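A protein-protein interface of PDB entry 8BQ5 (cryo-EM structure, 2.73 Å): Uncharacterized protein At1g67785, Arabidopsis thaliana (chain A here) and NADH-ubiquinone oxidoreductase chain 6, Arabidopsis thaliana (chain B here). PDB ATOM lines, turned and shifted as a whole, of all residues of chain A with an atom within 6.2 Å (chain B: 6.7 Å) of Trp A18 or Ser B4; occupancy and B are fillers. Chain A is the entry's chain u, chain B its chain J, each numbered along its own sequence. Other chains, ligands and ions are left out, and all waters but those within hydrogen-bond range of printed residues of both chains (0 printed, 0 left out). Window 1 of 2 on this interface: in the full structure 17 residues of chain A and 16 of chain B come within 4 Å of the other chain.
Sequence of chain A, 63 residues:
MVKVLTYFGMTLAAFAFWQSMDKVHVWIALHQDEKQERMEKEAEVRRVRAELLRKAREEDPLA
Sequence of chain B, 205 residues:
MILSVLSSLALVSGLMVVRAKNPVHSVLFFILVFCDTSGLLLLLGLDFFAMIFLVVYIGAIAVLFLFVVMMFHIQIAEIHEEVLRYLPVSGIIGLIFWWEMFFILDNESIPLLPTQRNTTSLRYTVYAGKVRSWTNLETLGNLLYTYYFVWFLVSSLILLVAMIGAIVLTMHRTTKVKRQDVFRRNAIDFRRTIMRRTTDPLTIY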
ATOM      1  N   ALA A  13     -17.338  12.018   5.263  1.00  0.00           N
ATOM      2  CA  ALA A  13     -17.402  11.574   3.875  1.00  0.00           C
ATOM      3  C   ALA A  13     -17.660  12.747   2.936  1.00  0.00           C
ATOM      4  O   ALA A  13     -17.035  12.856   1.874  1.00  0.00           O
ATOM      5  CB  ALA A  13     -18.483  10.508   3.717  1.00  0.00           C
ATOM      6  N   ALA A  14     -18.573  13.642   3.318  1.00  0.00           N
ATOM      7  CA  ALA A  14     -18.869  14.795   2.474  1.00  0.00           C
ATOM      8  C   ALA A  14     -17.682  15.750   2.401  1.00  0.00           C
ATOM      9  O   ALA A  14     -17.434  16.364   1.357  1.00  0.00           O
ATOM     10  CB  ALA A  14     -20.117  15.512   2.980  1.00  0.00           C
ATOM     11  N   PHE A  15     -16.935  15.893   3.497  1.00  0.00           N
ATOM     12  CA  PHE A  15     -15.727  16.713   3.451  1.00  0.00           C
ATOM     13  C   PHE A  15     -14.719  16.146   2.460  1.00  0.00           C
ATOM     14  O   PHE A  15     -14.111  16.893   1.677  1.00  0.00           O
ATOM     15  CB  PHE A  15     -15.104  16.824   4.841  1.00  0.00           C
ATOM     16  CG  PHE A  15     -13.880  17.683   4.873  1.00  0.00           C
ATOM     17  CD1 PHE A  15     -13.988  19.063   4.885  1.00  0.00           C
ATOM     18  CD2 PHE A  15     -12.618  17.114   4.853  1.00  0.00           C
ATOM     19  CE1 PHE A  15     -12.859  19.856   4.899  1.00  0.00           C
ATOM     20  CE2 PHE A  15     -11.489  17.901   4.866  1.00  0.00           C
ATOM     21  CZ  PHE A  15     -11.609  19.276   4.889  1.00  0.00           C
ATOM     22  N   ALA A  16     -14.533  14.824   2.478  1.00  0.00           N
ATOM     23  CA  ALA A  16     -13.649  14.197   1.500  1.00  0.00           C
ATOM     24  C   ALA A  16     -14.151  14.429   0.078  1.00  0.00           C
ATOM     25  O   ALA A  16     -13.359  14.690  -0.842  1.00  0.00           O
ATOM     26  CB  ALA A  16     -13.520  12.702   1.795  1.00  0.00           C
ATOM     27  N   PHE A  17     -15.470  14.355  -0.114  1.00  0.00           N
ATOM     28  CA  PHE A  17     -16.052  14.592  -1.432  1.00  0.00           C
ATOM     29  C   PHE A  17     -15.778  16.015  -1.913  1.00  0.00           C
ATOM     30  O   PHE A  17     -15.485  16.238  -3.094  1.00  0.00           O
ATOM     31  CB  PHE A  17     -17.555  14.303  -1.381  1.00  0.00           C
ATOM     32  CG  PHE A  17     -18.339  14.919  -2.503  1.00  0.00           C
ATOM     33  CD1 PHE A  17     -18.376  14.317  -3.750  1.00  0.00           C
ATOM     34  CD2 PHE A  17     -19.055  16.087  -2.306  1.00  0.00           C
ATOM     35  CE1 PHE A  17     -19.102  14.877  -4.782  1.00  0.00           C
ATOM     36  CE2 PHE A  17     -19.782  16.653  -3.336  1.00  0.00           C
ATOM     37  CZ  PHE A  17     -19.807  16.045  -4.575  1.00  0.00           C
ATOM     38  N   TRP A  18     -15.852  16.993  -1.007  1.00  0.00           N
ATOM     39  CA  TRP A  18     -15.613  18.378  -1.410  1.00  0.00           C
ATOM     40  C   TRP A  18     -14.140  18.627  -1.721  1.00  0.00           C
ATOM     41  O   TRP A  18     -13.816  19.379  -2.650  1.00  0.00           O
ATOM     42  CB  TRP A  18     -16.124  19.338  -0.337  1.00  0.00           C
ATOM     43  CG  TRP A  18     -17.615  19.397  -0.317  1.00  0.00           C
ATOM     44  CD1 TRP A  18     -18.436  19.003   0.696  1.00  0.00           C
ATOM     45  CD2 TRP A  18     -18.471  19.843  -1.376  1.00  0.00           C
ATOM     46  NE1 TRP A  18     -19.749  19.185   0.340  1.00  0.00           N
ATOM     47  CE2 TRP A  18     -19.797  19.702  -0.928  1.00  0.00           C
ATOM     48  CE3 TRP A  18     -18.243  20.357  -2.656  1.00  0.00           C
ATOM     49  CZ2 TRP A  18     -20.892  20.054  -1.713  1.00  0.00           C
ATOM     50  CZ3 TRP A  18     -19.330  20.707  -3.435  1.00  0.00           C
ATOM     51  CH2 TRP A  18     -20.637  20.554  -2.961  1.00  0.00           C
ATOM     52  N   GLN A  19     -13.229  18.001  -0.972  1.00  0.00           N
ATOM     53  CA  GLN A  19     -11.814  18.122  -1.323  1.00  0.00           C
ATOM     54  C   GLN A  19     -11.528  17.507  -2.695  1.00  0.00           C
ATOM     55  O   GLN A  19     -10.754  18.064  -3.493  1.00  0.00           O
ATOM     56  CB  GLN A  19     -10.943  17.489  -0.240  1.00  0.00           C
ATOM     57  CG  GLN A  19     -11.183  18.051   1.156  1.00  0.00           C
ATOM     58  CD  GLN A  19     -10.727  19.494   1.302  1.00  0.00           C
ATOM     59  OE1 GLN A  19     -11.362  20.416   0.789  1.00  0.00           O
ATOM     60  NE2 GLN A  19      -9.621  19.694   2.007  1.00  0.00           N
ATOM     61  N   SER A  20     -12.159  16.368  -2.996  1.00  0.00           N
ATOM     62  CA  SER A  20     -12.036  15.798  -4.336  1.00  0.00           C
ATOM     63  C   SER A  20     -12.582  16.751  -5.396  1.00  0.00           C
ATOM     64  O   SER A  20     -12.012  16.873  -6.489  1.00  0.00           O
ATOM     65  CB  SER A  20     -12.759  14.455  -4.405  1.00  0.00           C
ATOM     66  OG  SER A  20     -12.587  13.722  -3.207  1.00  0.00           O
ATOM     67  N   MET A  21     -13.694  17.423  -5.094  1.00  0.00           N
ATOM     68  CA  MET A  21     -14.229  18.418  -6.021  1.00  0.00           C
ATOM     69  C   MET A  21     -13.224  19.538  -6.264  1.00  0.00           C
ATOM     70  O   MET A  21     -13.107  20.050  -7.384  1.00  0.00           O
ATOM     71  CB  MET A  21     -15.544  18.983  -5.482  1.00  0.00           C
ATOM     72  CG  MET A  21     -16.776  18.224  -5.943  1.00  0.00           C
ATOM     73  SD  MET A  21     -16.733  17.840  -7.703  1.00  0.00           S
ATOM     74  CE  MET A  21     -16.981  16.069  -7.658  1.00  0.00           C
ATOM     75  N   ASP A  22     -12.498  19.939  -5.219  1.00  0.00           N
ATOM     76  CA  ASP A  22     -11.451  20.945  -5.388  1.00  0.00           C
ATOM     77  C   ASP A  22     -10.371  20.453  -6.346  1.00  0.00           C
ATOM     78  O   ASP A  22      -9.892  21.204  -7.209  1.00  0.00           O
ATOM     79  CB  ASP A  22     -10.842  21.305  -4.034  1.00  0.00           C
ATOM     80  CG  ASP A  22     -11.789  22.105  -3.169  1.00  0.00           C
ATOM     81  OD1 ASP A  22     -12.792  22.624  -3.704  1.00  0.00           O
ATOM     82  OD2 ASP A  22     -11.529  22.218  -1.953  1.00  0.00           O
ATOM     83  N   LYS A  23      -9.968  19.188  -6.198  1.00  0.00           N
ATOM     84  CA  LYS A  23      -8.996  18.620  -7.133  1.00  0.00           C
ATOM     85  C   LYS A  23      -9.525  18.658  -8.564  1.00  0.00           C
ATOM     86  O   LYS A  23      -8.785  18.972  -9.505  1.00  0.00           O
ATOM     87  CB  LYS A  23      -8.640  17.188  -6.732  1.00  0.00           C
ATOM     88  CG  LYS A  23      -7.817  17.080  -5.460  1.00  0.00           C
ATOM     89  CD  LYS A  23      -7.920  15.692  -4.840  1.00  0.00           C
ATOM     90  CE  LYS A  23      -6.546  15.073  -4.616  1.00  0.00           C
ATOM     91  NZ  LYS A  23      -6.558  13.590  -4.767  1.00  0.00           N
ATOM     92  N   MET B   1     -11.185  25.630   2.747  1.00  0.00           N
ATOM     93  CA  MET B   1     -11.328  24.619   3.787  1.00  0.00           C
ATOM     94  C   MET B   1     -12.601  24.849   4.596  1.00  0.00           C
ATOM     95  O   MET B   1     -13.381  23.923   4.808  1.00  0.00           O
ATOM     96  CB  MET B   1     -10.104  24.617   4.705  1.00  0.00           C
ATOM     97  CG  MET B   1     -10.027  23.432   5.652  1.00  0.00           C
ATOM     98  SD  MET B   1     -10.620  23.831   7.307  1.00  0.00           S
ATOM     99  CE  MET B   1      -9.243  24.789   7.942  1.00  0.00           C
ATOM    100  N   ILE B   2     -12.801  26.089   5.050  1.00  0.00           N
ATOM    101  CA  ILE B   2     -14.026  26.423   5.772  1.00  0.00           C
ATOM    102  C   ILE B   2     -15.235  26.251   4.863  1.00  0.00           C
ATOM    103  O   ILE B   2     -16.292  25.763   5.290  1.00  0.00           O
ATOM    104  CB  ILE B   2     -13.941  27.849   6.346  1.00  0.00           C
ATOM    105  CG1 ILE B   2     -12.878  27.915   7.443  1.00  0.00           C
ATOM    106  CG2 ILE B   2     -15.298  28.296   6.880  1.00  0.00           C
ATOM    107  CD1 ILE B   2     -13.066  29.063   8.416  1.00  0.00           C
ATOM    108  N   LEU B   3     -15.104  26.655   3.599  1.00  0.00           N
ATOM    109  CA  LEU B   3     -16.158  26.386   2.630  1.00  0.00           C
ATOM    110  C   LEU B   3     -16.389  24.894   2.460  1.00  0.00           C
ATOM    111  O   LEU B   3     -17.534  24.470   2.301  1.00  0.00           O
ATOM    112  CB  LEU B   3     -15.830  27.037   1.288  1.00  0.00           C
ATOM    113  CG  LEU B   3     -16.290  28.487   1.157  1.00  0.00           C
ATOM    114  CD1 LEU B   3     -15.295  29.299   0.352  1.00  0.00           C
ATOM    115  CD2 LEU B   3     -17.664  28.529   0.510  1.00  0.00           C
ATOM    116  N   SER B   4     -15.330  24.086   2.510  1.00  0.00           N
ATOM    117  CA  SER B   4     -15.515  22.640   2.465  1.00  0.00           C
ATOM    118  C   SER B   4     -16.306  22.144   3.673  1.00  0.00           C
ATOM    119  O   SER B   4     -17.191  21.293   3.531  1.00  0.00           O
ATOM    120  CB  SER B   4     -14.162  21.937   2.379  1.00  0.00           C
ATOM    121  OG  SER B   4     -13.719  21.857   1.036  1.00  0.00           O
ATOM    122  N   VAL B   5     -16.014  22.674   4.864  1.00  0.00           N
ATOM    123  CA  VAL B   5     -16.724  22.240   6.066  1.00  0.00           C
ATOM    124  C   VAL B   5     -18.201  22.604   5.978  1.00  0.00           C
ATOM    125  O   VAL B   5     -19.083  21.765   6.213  1.00  0.00           O
ATOM    126  CB  VAL B   5     -16.073  22.843   7.324  1.00  0.00           C
ATOM    127  CG1 VAL B   5     -16.976  22.647   8.530  1.00  0.00           C
ATOM    128  CG2 VAL B   5     -14.719  22.209   7.576  1.00  0.00           C
ATOM    129  N   LEU B   6     -18.494  23.863   5.640  1.00  0.00           N
ATOM    130  CA  LEU B   6     -19.888  24.280   5.522  1.00  0.00           C
ATOM    131  C   LEU B   6     -20.595  23.514   4.410  1.00  0.00           C
ATOM    132  O   LEU B   6     -21.753  23.116   4.562  1.00  0.00           O
ATOM    133  CB  LEU B   6     -19.980  25.789   5.290  1.00  0.00           C
ATOM    134  CG  LEU B   6     -19.619  26.725   6.450  1.00  0.00           C
ATOM    135  CD1 LEU B   6     -20.068  28.143   6.151  1.00  0.00           C
ATOM    136  CD2 LEU B   6     -20.223  26.253   7.763  1.00  0.00           C
ATOM    137  N   SER B   7     -19.915  23.282   3.289  1.00  0.00           N
ATOM    138  CA  SER B   7     -20.528  22.526   2.205  1.00  0.00           C
ATOM    139  C   SER B   7     -20.875  21.111   2.647  1.00  0.00           C
ATOM    140  O   SER B   7     -21.952  20.604   2.319  1.00  0.00           O
ATOM    141  CB  SER B   7     -19.593  22.504   0.997  1.00  0.00           C
ATOM    142  OG  SER B   7     -19.570  23.765   0.351  1.00  0.00           O
ATOM    143  N   SER B   8     -19.984  20.462   3.400  1.00  0.00           N
ATOM    144  CA  SER B   8     -20.260  19.108   3.870  1.00  0.00           C
ATOM    145  C   SER B   8     -21.424  19.085   4.855  1.00  0.00           C
ATOM    146  O   SER B   8     -22.297  18.207   4.780  1.00  0.00           O
ATOM    147  CB  SER B   8     -19.005  18.511   4.505  1.00  0.00           C
ATOM    148  OG  SER B   8     -18.934  18.828   5.883  1.00  0.00           O
ATOM    149  N   LEU B   9     -21.451  20.041   5.787  1.00  0.00           N
ATOM    150  CA  LEU B   9     -22.554  20.101   6.740  1.00  0.00           C
ATOM    151  C   LEU B   9     -23.882  20.326   6.028  1.00  0.00           C
ATOM    152  O   LEU B   9     -24.884  19.677   6.348  1.00  0.00           O
ATOM    153  CB  LEU B   9     -22.300  21.194   7.778  1.00  0.00           C
ATOM    154  CG  LEU B   9     -21.343  20.817   8.911  1.00  0.00           C
ATOM    155  CD1 LEU B   9     -21.073  22.006   9.814  1.00  0.00           C
ATOM    156  CD2 LEU B   9     -21.894  19.651   9.713  1.00  0.00           C
ATOM    157  N   ALA B  10     -23.903  21.225   5.041  1.00  0.00           N
ATOM    158  CA  ALA B  10     -25.133  21.475   4.297  1.00  0.00           C
ATOM    159  C   ALA B  10     -25.546  20.258   3.483  1.00  0.00           C
ATOM    160  O   ALA B  10     -26.735  19.939   3.398  1.00  0.00           O
ATOM    161  CB  ALA B  10     -24.969  22.693   3.392  1.00  0.00           C
ATOM    162  N   LEU B  11     -24.580  19.563   2.880  1.00  0.00           N
ATOM    163  CA  LEU B  11     -24.902  18.373   2.101  1.00  0.00           C
ATOM    164  C   LEU B  11     -25.569  17.322   2.982  1.00  0.00           C
ATOM    165  O   LEU B  11     -26.627  16.782   2.635  1.00  0.00           O
ATOM    166  CB  LEU B  11     -23.626  17.820   1.457  1.00  0.00           C
ATOM    167  CG  LEU B  11     -23.664  16.804   0.305  1.00  0.00           C
ATOM    168  CD1 LEU B  11     -22.259  16.331  -0.017  1.00  0.00           C
ATOM    169  CD2 LEU B  11     -24.533  15.624   0.562  1.00  0.00           C
ATOM    170  N   PHE B 102     -22.502  21.724 -12.011  1.00  0.00           N
ATOM    171  CA  PHE B 102     -21.460  22.112 -11.066  1.00  0.00           C
ATOM    172  C   PHE B 102     -20.254  22.748 -11.741  1.00  0.00           C
ATOM    173  O   PHE B 102     -19.429  23.359 -11.053  1.00  0.00           O
ATOM    174  CB  PHE B 102     -20.995  20.909 -10.237  1.00  0.00           C
ATOM    175  CG  PHE B 102     -22.004  20.421  -9.239  1.00  0.00           C
ATOM    176  CD1 PHE B 102     -21.761  20.551  -7.884  1.00  0.00           C
ATOM    177  CD2 PHE B 102     -23.191  19.847  -9.643  1.00  0.00           C
ATOM    178  CE1 PHE B 102     -22.678  20.107  -6.954  1.00  0.00           C
ATOM    179  CE2 PHE B 102     -24.113  19.397  -8.719  1.00  0.00           C
ATOM    180  CZ  PHE B 102     -23.856  19.531  -7.373  1.00  0.00           C
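OG of Ser B7 lies within hydrogen-bond range of O of Leu B3. The backbone carbonyl oxygen (O) of Val B5 sits at hydrogen-bond distance from the side-chain hydroxyl (OG) of Ser B8, at 3.0 Å. OE1 of Gln A19 sits close to OD2 of Asp A22, 3.3 Å away.
Hydrophobic or aromatic side chains of chain B within 4 Å of the printed part of chain A: Leu B11. Along chain B the printed residues that touch a printed residue of chain A span positions 4 to 11. Among the printed residues, no Asp or Glu carboxylate lies within 4 Å of a Lys or Arg side-chain nitrogen of the other chain.
The side-chain hydroxyl of Ser B4 lies within hydrogen-bond range of the side-chain amide oxygen of Gln A19, at 2.8 Å. NE1 of Trp A18 sits close to O of Ser B7 (3.3 Å). NE1 of Trp A18 lies close to N of Ser B8.
Of chain B, only Ser B4 (3.7 Å), Ser B7 (3.2 Å), Ser B8 (3.3 Å) and Leu B11 (3.8 Å) come within 4 Å of Trp A18. Of the printed residues of chain A, Leu B11 touches Ala A14, Phe A17 and Trp A18. Of the printed residues of chain A, Ser B8 touches Ala A14, Phe A15 and Trp A18. Met A21 touches none of the printed residues of chain B.
Among the printed residues, pairs that only touch across the chains: Ala A14 with Ser B8 (3.5 Å), Ala A14 with Leu B11 (3.8 Å), Phe A15 with Ser B4 (3.5 Å), Phe A15 with Ser B8 (3.5 Å), Phe A17 with Leu B11 (3.9 Å), Trp A18 with Ser B4 (3.7 Å), Trp A18 with Leu B11 (3.8 Å) and Asp A22 with Ser B4 (3.7 Å).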
